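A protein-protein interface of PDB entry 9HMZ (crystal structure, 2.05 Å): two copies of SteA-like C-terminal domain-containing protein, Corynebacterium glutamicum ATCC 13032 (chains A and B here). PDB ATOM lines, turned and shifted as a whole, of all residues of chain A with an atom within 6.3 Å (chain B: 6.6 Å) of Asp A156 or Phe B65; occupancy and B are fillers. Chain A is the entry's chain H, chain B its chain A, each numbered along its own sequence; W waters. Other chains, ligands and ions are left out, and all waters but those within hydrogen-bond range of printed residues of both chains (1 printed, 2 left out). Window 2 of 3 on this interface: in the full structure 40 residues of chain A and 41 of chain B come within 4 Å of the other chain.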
ATOM      1  N   ALA A 151      -5.492  21.195 -19.182  1.00  0.00           N
ATOM      2  CA  ALA A 151      -6.374  21.446 -18.047  1.00  0.00           C
ATOM      3  C   ALA A 151      -6.784  22.927 -17.962  1.00  0.00           C
ATOM      4  O   ALA A 151      -7.959  23.154 -17.737  1.00  0.00           O
ATOM      5  CB  ALA A 151      -5.733  20.992 -16.745  1.00  0.00           C
ATOM      6  N   PRO A 152      -5.914  23.953 -18.198  1.00  0.00           N
ATOM      7  CA  PRO A 152      -6.407  25.352 -18.171  1.00  0.00           C
ATOM      8  C   PRO A 152      -7.626  25.602 -19.063  1.00  0.00           C
ATOM      9  O   PRO A 152      -8.506  26.372 -18.692  1.00  0.00           O
ATOM     10  CB  PRO A 152      -5.200  26.172 -18.658  1.00  0.00           C
ATOM     11  CG  PRO A 152      -4.039  25.361 -18.304  1.00  0.00           C
ATOM     12  CD  PRO A 152      -4.456  23.922 -18.453  1.00  0.00           C
ATOM     13  N   LEU A 153      -7.690  24.941 -20.218  1.00  0.00           N
ATOM     14  CA  LEU A 153      -8.805  25.082 -21.122  1.00  0.00           C
ATOM     15  C   LEU A 153     -10.019  24.263 -20.638  1.00  0.00           C
ATOM     16  O   LEU A 153     -11.121  24.797 -20.569  1.00  0.00           O
ATOM     17  CB  LEU A 153      -8.374  24.655 -22.528  1.00  0.00           C
ATOM     18  CG  LEU A 153      -9.501  24.543 -23.536  1.00  0.00           C
ATOM     19  CD1 LEU A 153     -10.119  25.922 -23.812  1.00  0.00           C
ATOM     20  CD2 LEU A 153      -9.032  23.828 -24.799  1.00  0.00           C
ATOM     21  N   LEU A 154      -9.828  22.970 -20.335  1.00  0.00           N
ATOM     22  CA  LEU A 154     -10.911  22.084 -19.902  1.00  0.00           C
ATOM     23  C   LEU A 154     -11.517  22.450 -18.580  1.00  0.00           C
ATOM     24  O   LEU A 154     -12.714  22.258 -18.415  1.00  0.00           O
ATOM     25  CB  LEU A 154     -10.406  20.656 -19.829  1.00  0.00           C
ATOM     26  CG  LEU A 154     -10.084  19.986 -21.142  1.00  0.00           C
ATOM     27  CD1 LEU A 154      -9.331  18.641 -20.896  1.00  0.00           C
ATOM     28  CD2 LEU A 154     -11.362  19.768 -21.926  1.00  0.00           C
ATOM     29  N   ILE A 155     -10.711  22.950 -17.617  1.00  0.00           N
ATOM     30  CA  ILE A 155     -11.169  23.307 -16.283  1.00  0.00           C
ATOM     31  C   ILE A 155     -11.525  24.774 -16.199  1.00  0.00           C
ATOM     32  O   ILE A 155     -12.617  25.095 -15.725  1.00  0.00           O
ATOM     33  CB  ILE A 155     -10.090  22.942 -15.196  1.00  0.00           C
ATOM     34  CG1 ILE A 155      -9.760  21.433 -15.188  1.00  0.00           C
ATOM     35  CG2 ILE A 155     -10.446  23.472 -13.782  1.00  0.00           C
ATOM     36  CD1 ILE A 155     -10.794  20.611 -14.849  1.00  0.00           C
ATOM     37  N   ASP A 156     -10.613  25.684 -16.610  1.00  0.00           N
ATOM     38  CA  ASP A 156     -10.880  27.113 -16.458  1.00  0.00           C
ATOM     39  C   ASP A 156     -11.409  27.845 -17.645  1.00  0.00           C
ATOM     40  O   ASP A 156     -11.767  29.016 -17.500  1.00  0.00           O
ATOM     41  CB  ASP A 156      -9.635  27.850 -15.991  1.00  0.00           C
ATOM     42  CG  ASP A 156      -9.323  27.673 -14.530  1.00  0.00           C
ATOM     43  OD1 ASP A 156     -10.267  27.399 -13.747  1.00  0.00           O
ATOM     44  OD2 ASP A 156      -8.151  27.843 -14.162  1.00  0.00           O
ATOM     45  N   GLY A 157     -11.388  27.225 -18.811  1.00  0.00           N
ATOM     46  CA  GLY A 157     -11.802  27.922 -20.017  1.00  0.00           C
ATOM     47  C   GLY A 157     -10.792  28.985 -20.419  1.00  0.00           C
ATOM     48  O   GLY A 157     -11.178  29.989 -21.020  1.00  0.00           O
ATOM     49  N   LEU A 158      -9.491  28.787 -20.090  1.00  0.00           N
ATOM     50  CA  LEU A 158      -8.420  29.700 -20.468  1.00  0.00           C
ATOM     51  C   LEU A 158      -8.336  29.780 -21.975  1.00  0.00           C
ATOM     52  O   LEU A 158      -8.332  28.750 -22.656  1.00  0.00           O
ATOM     53  CB  LEU A 158      -7.052  29.255 -19.916  1.00  0.00           C
ATOM     54  CG  LEU A 158      -5.816  30.075 -20.432  1.00  0.00           C
ATOM     55  CD1 LEU A 158      -5.601  31.322 -19.632  1.00  0.00           C
ATOM     56  CD2 LEU A 158      -4.542  29.257 -20.456  1.00  0.00           C
ATOM     57  N   ILE A 160     -10.656  30.948 -23.971  1.00  0.00           N
ATOM     58  CA  ILE A 160     -11.980  31.085 -24.574  1.00  0.00           C
ATOM     59  C   ILE A 160     -12.409  32.540 -24.578  1.00  0.00           C
ATOM     60  O   ILE A 160     -12.432  33.172 -23.535  1.00  0.00           O
ATOM     61  CB  ILE A 160     -13.051  30.178 -23.909  1.00  0.00           C
ATOM     62  CG1 ILE A 160     -12.638  28.691 -23.933  1.00  0.00           C
ATOM     63  CG2 ILE A 160     -14.417  30.376 -24.566  1.00  0.00           C
ATOM     64  CD1 ILE A 160     -13.555  27.734 -23.203  1.00  0.00           C
ATOM     65  N   PHE A 280     -18.873  27.023 -22.667  1.00  0.00           N
ATOM     66  CA  PHE A 280     -18.358  27.983 -21.697  1.00  0.00           C
ATOM     67  C   PHE A 280     -19.325  29.143 -21.433  1.00  0.00           C
ATOM     68  O   PHE A 280     -19.339  29.702 -20.336  1.00  0.00           O
ATOM     69  CB  PHE A 280     -17.006  28.507 -22.168  1.00  0.00           C
ATOM     70  CG  PHE A 280     -16.303  29.318 -21.113  1.00  0.00           C
ATOM     71  CD1 PHE A 280     -15.796  28.713 -19.973  1.00  0.00           C
ATOM     72  CD2 PHE A 280     -16.143  30.681 -21.263  1.00  0.00           C
ATOM     73  CE1 PHE A 280     -15.144  29.458 -19.005  1.00  0.00           C
ATOM     74  CE2 PHE A 280     -15.483  31.421 -20.297  1.00  0.00           C
ATOM     75  CZ  PHE A 280     -14.994  30.810 -19.171  1.00  0.00           C
ATOM     76  N   ASP B  34     -13.348  26.064  -5.045  1.00  0.00           N
ATOM     77  CA  ASP B  34     -12.824  25.885  -6.395  1.00  0.00           C
ATOM     78  C   ASP B  34     -13.288  27.018  -7.333  1.00  0.00           C
ATOM     79  O   ASP B  34     -13.836  26.759  -8.410  1.00  0.00           O
ATOM     80  CB  ASP B  34     -13.165  24.499  -6.940  1.00  0.00           C
ATOM     81  CG  ASP B  34     -12.421  23.409  -6.208  1.00  0.00           C
ATOM     82  OD1 ASP B  34     -11.249  23.631  -5.858  1.00  0.00           O
ATOM     83  OD2 ASP B  34     -13.013  22.327  -5.985  1.00  0.00           O
ATOM     84  N   LEU B  35     -13.082  28.277  -6.874  1.00  0.00           N
ATOM     85  CA  LEU B  35     -13.435  29.517  -7.545  1.00  0.00           C
ATOM     86  C   LEU B  35     -13.211  29.470  -9.072  1.00  0.00           C
ATOM     87  O   LEU B  35     -12.096  29.189  -9.521  1.00  0.00           O
ATOM     88  CB  LEU B  35     -12.651  30.676  -6.919  1.00  0.00           C
ATOM     89  CG  LEU B  35     -12.899  32.045  -7.552  1.00  0.00           C
ATOM     90  CD1 LEU B  35     -14.274  32.585  -7.177  1.00  0.00           C
ATOM     91  CD2 LEU B  35     -11.815  33.017  -7.164  1.00  0.00           C
ATOM     92  N   SER B  36     -14.287  29.685  -9.855  1.00  0.00           N
ATOM     93  CA  SER B  36     -14.204  29.656 -11.306  1.00  0.00           C
ATOM     94  C   SER B  36     -13.506  30.898 -11.860  1.00  0.00           C
ATOM     95  O   SER B  36     -13.465  31.935 -11.196  1.00  0.00           O
ATOM     96  CB  SER B  36     -15.585  29.491 -11.934  1.00  0.00           C
ATOM     97  OG  SER B  36     -16.381  30.655 -11.787  1.00  0.00           O
ATOM     98  N   ARG B  37     -12.926  30.778 -13.069  1.00  0.00           N
ATOM     99  CA  ARG B  37     -12.228  31.876 -13.726  1.00  0.00           C
ATOM    100  C   ARG B  37     -13.198  33.007 -14.035  1.00  0.00           C
ATOM    101  O   ARG B  37     -12.837  34.166 -13.859  1.00  0.00           O
ATOM    102  CB  ARG B  37     -11.554  31.364 -15.003  1.00  0.00           C
ATOM    103  CG  ARG B  37     -10.845  32.438 -15.829  1.00  0.00           C
ATOM    104  CD  ARG B  37     -10.228  31.894 -17.116  1.00  0.00           C
ATOM    105  NE  ARG B  37      -9.182  30.900 -16.835  1.00  0.00           N
ATOM    106  CZ  ARG B  37      -7.879  31.164 -16.813  1.00  0.00           C
ATOM    107  NH1 ARG B  37      -7.441  32.392 -17.063  1.00  0.00           N
ATOM    108  NH2 ARG B  37      -7.004  30.203 -16.532  1.00  0.00           N
ATOM    109  N   THR B  38     -14.444  32.673 -14.450  1.00  0.00           N
ATOM    110  CA  THR B  38     -15.473  33.663 -14.740  1.00  0.00           C
ATOM    111  C   THR B  38     -15.835  34.501 -13.513  1.00  0.00           C
ATOM    112  O   THR B  38     -15.865  35.730 -13.609  1.00  0.00           O
ATOM    113  CB  THR B  38     -16.693  32.999 -15.374  1.00  0.00           C
ATOM    114  OG1 THR B  38     -16.283  32.392 -16.601  1.00  0.00           O
ATOM    115  CG2 THR B  38     -17.792  34.001 -15.702  1.00  0.00           C
ATOM    116  N   ALA B  40     -13.969  34.817 -10.763  1.00  0.00           N
ATOM    117  CA  ALA B  40     -12.754  35.537 -10.378  1.00  0.00           C
ATOM    118  C   ALA B  40     -12.534  36.781 -11.238  1.00  0.00           C
ATOM    119  O   ALA B  40     -12.048  37.789 -10.730  1.00  0.00           O
ATOM    120  CB  ALA B  40     -11.550  34.633 -10.497  1.00  0.00           C
ATOM    121  N   THR B  58      -9.078  26.757  -3.482  1.00  0.00           N
ATOM    122  CA  THR B  58      -8.661  25.573  -4.221  1.00  0.00           C
ATOM    123  C   THR B  58      -8.808  24.405  -3.260  1.00  0.00           C
ATOM    124  O   THR B  58      -8.053  24.322  -2.287  1.00  0.00           O
ATOM    125  CB  THR B  58      -7.214  25.730  -4.706  1.00  0.00           C
ATOM    126  OG1 THR B  58      -7.125  26.841  -5.611  1.00  0.00           O
ATOM    127  CG2 THR B  58      -6.637  24.440  -5.336  1.00  0.00           C
ATOM    128  N   VAL B  62      -9.129  20.129  -8.559  1.00  0.00           N
ATOM    129  CA  VAL B  62      -8.788  20.689  -9.880  1.00  0.00           C
ATOM    130  C   VAL B  62      -7.876  21.918  -9.822  1.00  0.00           C
ATOM    131  O   VAL B  62      -8.045  22.797  -8.963  1.00  0.00           O
ATOM    132  CB  VAL B  62     -10.052  20.998 -10.747  1.00  0.00           C
ATOM    133  CG1 VAL B  62     -10.806  19.717 -11.133  1.00  0.00           C
ATOM    134  CG2 VAL B  62     -10.970  22.009 -10.063  1.00  0.00           C
ATOM    135  N   PRO B  63      -6.935  22.038 -10.784  1.00  0.00           N
ATOM    136  CA  PRO B  63      -6.088  23.244 -10.811  1.00  0.00           C
ATOM    137  C   PRO B  63      -6.846  24.484 -11.317  1.00  0.00           C
ATOM    138  O   PRO B  63      -6.998  24.678 -12.526  1.00  0.00           O
ATOM    139  CB  PRO B  63      -4.922  22.835 -11.717  1.00  0.00           C
ATOM    140  CG  PRO B  63      -5.473  21.753 -12.598  1.00  0.00           C
ATOM    141  CD  PRO B  63      -6.600  21.089 -11.869  1.00  0.00           C
ATOM    142  N   ASN B  64      -7.317  25.327 -10.415  1.00  0.00           N
ATOM    143  CA  ASN B  64      -8.070  26.524 -10.791  1.00  0.00           C
ATOM    144  C   ASN B  64      -7.228  27.818 -10.605  1.00  0.00           C
ATOM    145  O   ASN B  64      -6.747  28.103  -9.517  1.00  0.00           O
ATOM    146  CB  ASN B  64      -9.438  26.578 -10.075  1.00  0.00           C
ATOM    147  CG  ASN B  64      -9.348  26.709  -8.593  1.00  0.00           C
ATOM    148  OD1 ASN B  64      -8.553  26.059  -7.956  1.00  0.00           O
ATOM    149  ND2 ASN B  64     -10.150  27.567  -8.005  1.00  0.00           N
ATOM    150  N   PHE B  65      -7.047  28.587 -11.694  1.00  0.00           N
ATOM    151  CA  PHE B  65      -6.227  29.783 -11.682  1.00  0.00           C
ATOM    152  C   PHE B  65      -6.887  31.034 -11.071  1.00  0.00           C
ATOM    153  O   PHE B  65      -6.173  31.939 -10.636  1.00  0.00           O
ATOM    154  CB  PHE B  65      -5.723  30.083 -13.081  1.00  0.00           C
ATOM    155  CG  PHE B  65      -4.538  31.007 -13.083  1.00  0.00           C
ATOM    156  CD1 PHE B  65      -3.314  30.583 -12.607  1.00  0.00           C
ATOM    157  CD2 PHE B  65      -4.650  32.303 -13.566  1.00  0.00           C
ATOM    158  CE1 PHE B  65      -2.218  31.432 -12.618  1.00  0.00           C
ATOM    159  CE2 PHE B  65      -3.547  33.150 -13.591  1.00  0.00           C
ATOM    160  CZ  PHE B  65      -2.334  32.703 -13.136  1.00  0.00           C
ATOM    161  N   GLY B  66      -8.225  31.062 -11.006  1.00  0.00           N
ATOM    162  CA  GLY B  66      -9.003  32.144 -10.398  1.00  0.00           C
ATOM    163  C   GLY B  66      -8.417  32.808  -9.153  1.00  0.00           C
ATOM    164  O   GLY B  66      -8.205  34.026  -9.165  1.00  0.00           O
ATOM    165  N   PRO B  67      -8.094  32.049  -8.069  1.00  0.00           N
ATOM    166  CA  PRO B  67      -7.483  32.682  -6.883  1.00  0.00           C
ATOM    167  C   PRO B  67      -6.188  33.455  -7.175  1.00  0.00           C
ATOM    168  O   PRO B  67      -6.001  34.536  -6.643  1.00  0.00           O
ATOM    169  CB  PRO B  67      -7.250  31.506  -5.924  1.00  0.00           C
ATOM    170  CG  PRO B  67      -8.202  30.448  -6.379  1.00  0.00           C
ATOM    171  CD  PRO B  67      -8.280  30.601  -7.864  1.00  0.00           C
ATOM    172  N   GLN B  68      -5.317  32.932  -8.043  1.00  0.00           N
ATOM    173  CA  GLN B  68      -4.084  33.615  -8.427  1.00  0.00           C
ATOM    174  C   GLN B  68      -4.337  34.888  -9.207  1.00  0.00           C
ATOM    175  O   GLN B  68      -3.572  35.834  -9.068  1.00  0.00           O
ATOM    176  CB  GLN B  68      -3.140  32.693  -9.187  1.00  0.00           C
ATOM    177  CG  GLN B  68      -2.519  31.631  -8.299  1.00  0.00           C
ATOM    178  CD  GLN B  68      -1.754  30.620  -9.109  1.00  0.00           C
ATOM    179  OE1 GLN B  68      -0.622  30.845  -9.513  1.00  0.00           O
ATOM    180  NE2 GLN B  68      -2.357  29.482  -9.376  1.00  0.00           N
ATOM    181  N   MET B  69      -5.408  34.947  -9.997  1.00  0.00           N
ATOM    182  CA  MET B  69      -5.755  36.167 -10.736  1.00  0.00           C
ATOM    183  C   MET B  69      -6.096  37.294  -9.752  1.00  0.00           C
ATOM    184  O   MET B  69      -5.737  38.449  -9.985  1.00  0.00           O
ATOM    185  CB  MET B  69      -6.977  35.937 -11.627  1.00  0.00           C
ATOM    186  CG  MET B  69      -6.693  35.214 -12.877  1.00  0.00           C
ATOM    187  SD  MET B  69      -8.243  34.823 -13.739  1.00  0.00           S
ATOM    188  CE  MET B  69      -9.024  36.419 -13.742  1.00  0.00           C
ATOM    189  N   LEU B  70      -6.835  36.959  -8.687  1.00  0.00           N
ATOM    190  CA  LEU B  70      -7.231  37.908  -7.658  1.00  0.00           C
ATOM    191  C   LEU B  70      -6.012  38.435  -6.921  1.00  0.00           C
ATOM    192  O   LEU B  70      -5.876  39.643  -6.768  1.00  0.00           O
ATOM    193  CB  LEU B  70      -8.214  37.256  -6.680  1.00  0.00           C
ATOM    194  CG  LEU B  70      -9.595  36.896  -7.248  1.00  0.00           C
ATOM    195  CD1 LEU B  70     -10.481  36.314  -6.164  1.00  0.00           C
ATOM    196  CD2 LEU B  70     -10.271  38.102  -7.854  1.00  0.00           C
ATOM    197  N   ASP B  72      -2.863  38.440  -8.038  1.00  0.00           N
ATOM    198  CA  ASP B  72      -2.113  39.258  -8.989  1.00  0.00           C
ATOM    199  C   ASP B  72      -2.704  40.678  -9.139  1.00  0.00           C
ATOM    200  O   ASP B  72      -1.979  41.629  -9.476  1.00  0.00           O
ATOM    201  CB  ASP B  72      -2.047  38.591 -10.374  1.00  0.00           C
ATOM    202  CG  ASP B  72      -1.123  37.396 -10.474  1.00  0.00           C
ATOM    203  OD1 ASP B  72      -0.202  37.288  -9.634  1.00  0.00           O
ATOM    204  OD2 ASP B  72      -1.313  36.572 -11.410  1.00  0.00           O
ATOM    205  N   PHE B 125      -2.386  25.153  -6.311  1.00  0.00           N
ATOM    206  CA  PHE B 125      -2.664  24.920  -7.731  1.00  0.00           C
ATOM    207  C   PHE B 125      -1.806  23.769  -8.265  1.00  0.00           C
ATOM    208  O   PHE B 125      -2.342  22.862  -8.902  1.00  0.00           O
ATOM    209  CB  PHE B 125      -2.374  26.190  -8.536  1.00  0.00           C
ATOM    210  CG  PHE B 125      -2.675  26.100 -10.019  1.00  0.00           C
ATOM    211  CD1 PHE B 125      -1.724  25.642 -10.910  1.00  0.00           C
ATOM    212  CD2 PHE B 125      -3.890  26.526 -10.524  1.00  0.00           C
ATOM    213  CE1 PHE B 125      -2.010  25.556 -12.260  1.00  0.00           C
ATOM    214  CE2 PHE B 125      -4.144  26.489 -11.886  1.00  0.00           C
ATOM    215  CZ  PHE B 125      -3.216  25.985 -12.737  1.00  0.00           C
HETATM  216  O   HOH W   1     -12.950  27.461 -13.820  1.00  0.00           O
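Ile A155 touches Val B62.
Ile A155 touches Pro B63.
OD2 of Asp A156 touches O of Pro B63, 3.7 Å away.
Asn B64 touches Asp A156 (CA to OD2, 3.6 Å).
CD1 of Leu A158 touches NH1 of Arg B37 (3.3 Å).
CZ of Phe A280 touches OG1 of Thr B38, 3.3 Å away.
Water W1 lies within hydrogen-bond range of OD1 of Asp A156 (2.7 Å), O of Ile A155 (3.1 Å) and N of Arg B37 (3.4 Å).
O of Leu B35 is in hydrogen-bond range of ND2 of Asn B64 (3.0 Å).
OD1 of Asn B64 sits at hydrogen-bond distance from OG1 of Thr B58.
The backbone carbonyl oxygen (O) of Val B62 lies close to the side-chain amide oxygen (OD1) of Asn B64, 3.5 Å away.
The backbone NH (N) of Leu A158 is in hydrogen-bond range of the backbone carbonyl oxygen (O) of Pro A152 (3.0 Å).
Printed residues of chain B that touch a printed residue of chain A: Arg B37, Thr B38, Val B62, Pro B63, Asn B64 and Phe B65.
Along chain A the printed residues that touch a printed residue of chain B span positions 155 to 280.
Among the printed residues, Asp or Glu carboxylates within 4 Å of a Lys or Arg side-chain nitrogen of the other chain: Asp A156 with Arg B37.
No position is printed for both chains.
Of the 8 pairs that touch across the chains among the printed residues, none has its exchanged pair printed and touching as well.
Printed residues of chain B within 4 Å of Leu A158: Arg B37 (3.3 Å).
Of the printed residues of chain A, Arg B37 touches Asp A156 and Leu A158.
Of the printed residues of chain A, Thr B38 touches Phe A280.
Of the printed residues of chain A, Pro B63 touches Ile A155 (3.9 Å) and Asp A156 (3.7 Å).
Printed residues of chain A within 4 Å of Asn B64: Asp A156.
The nearest residue of chain A that does not touch Phe B65 is Leu A158 (6.2 Å).
The guanidinium group of Arg B37 lies within salt-bridge range of the side-chain carboxylate of Asp A156, 3.5 Å away.
The backbone NH (N) of Phe B65 lies within hydrogen-bond range of the side-chain carboxylate (OD2) of Asp A156, at 2.8 Å.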
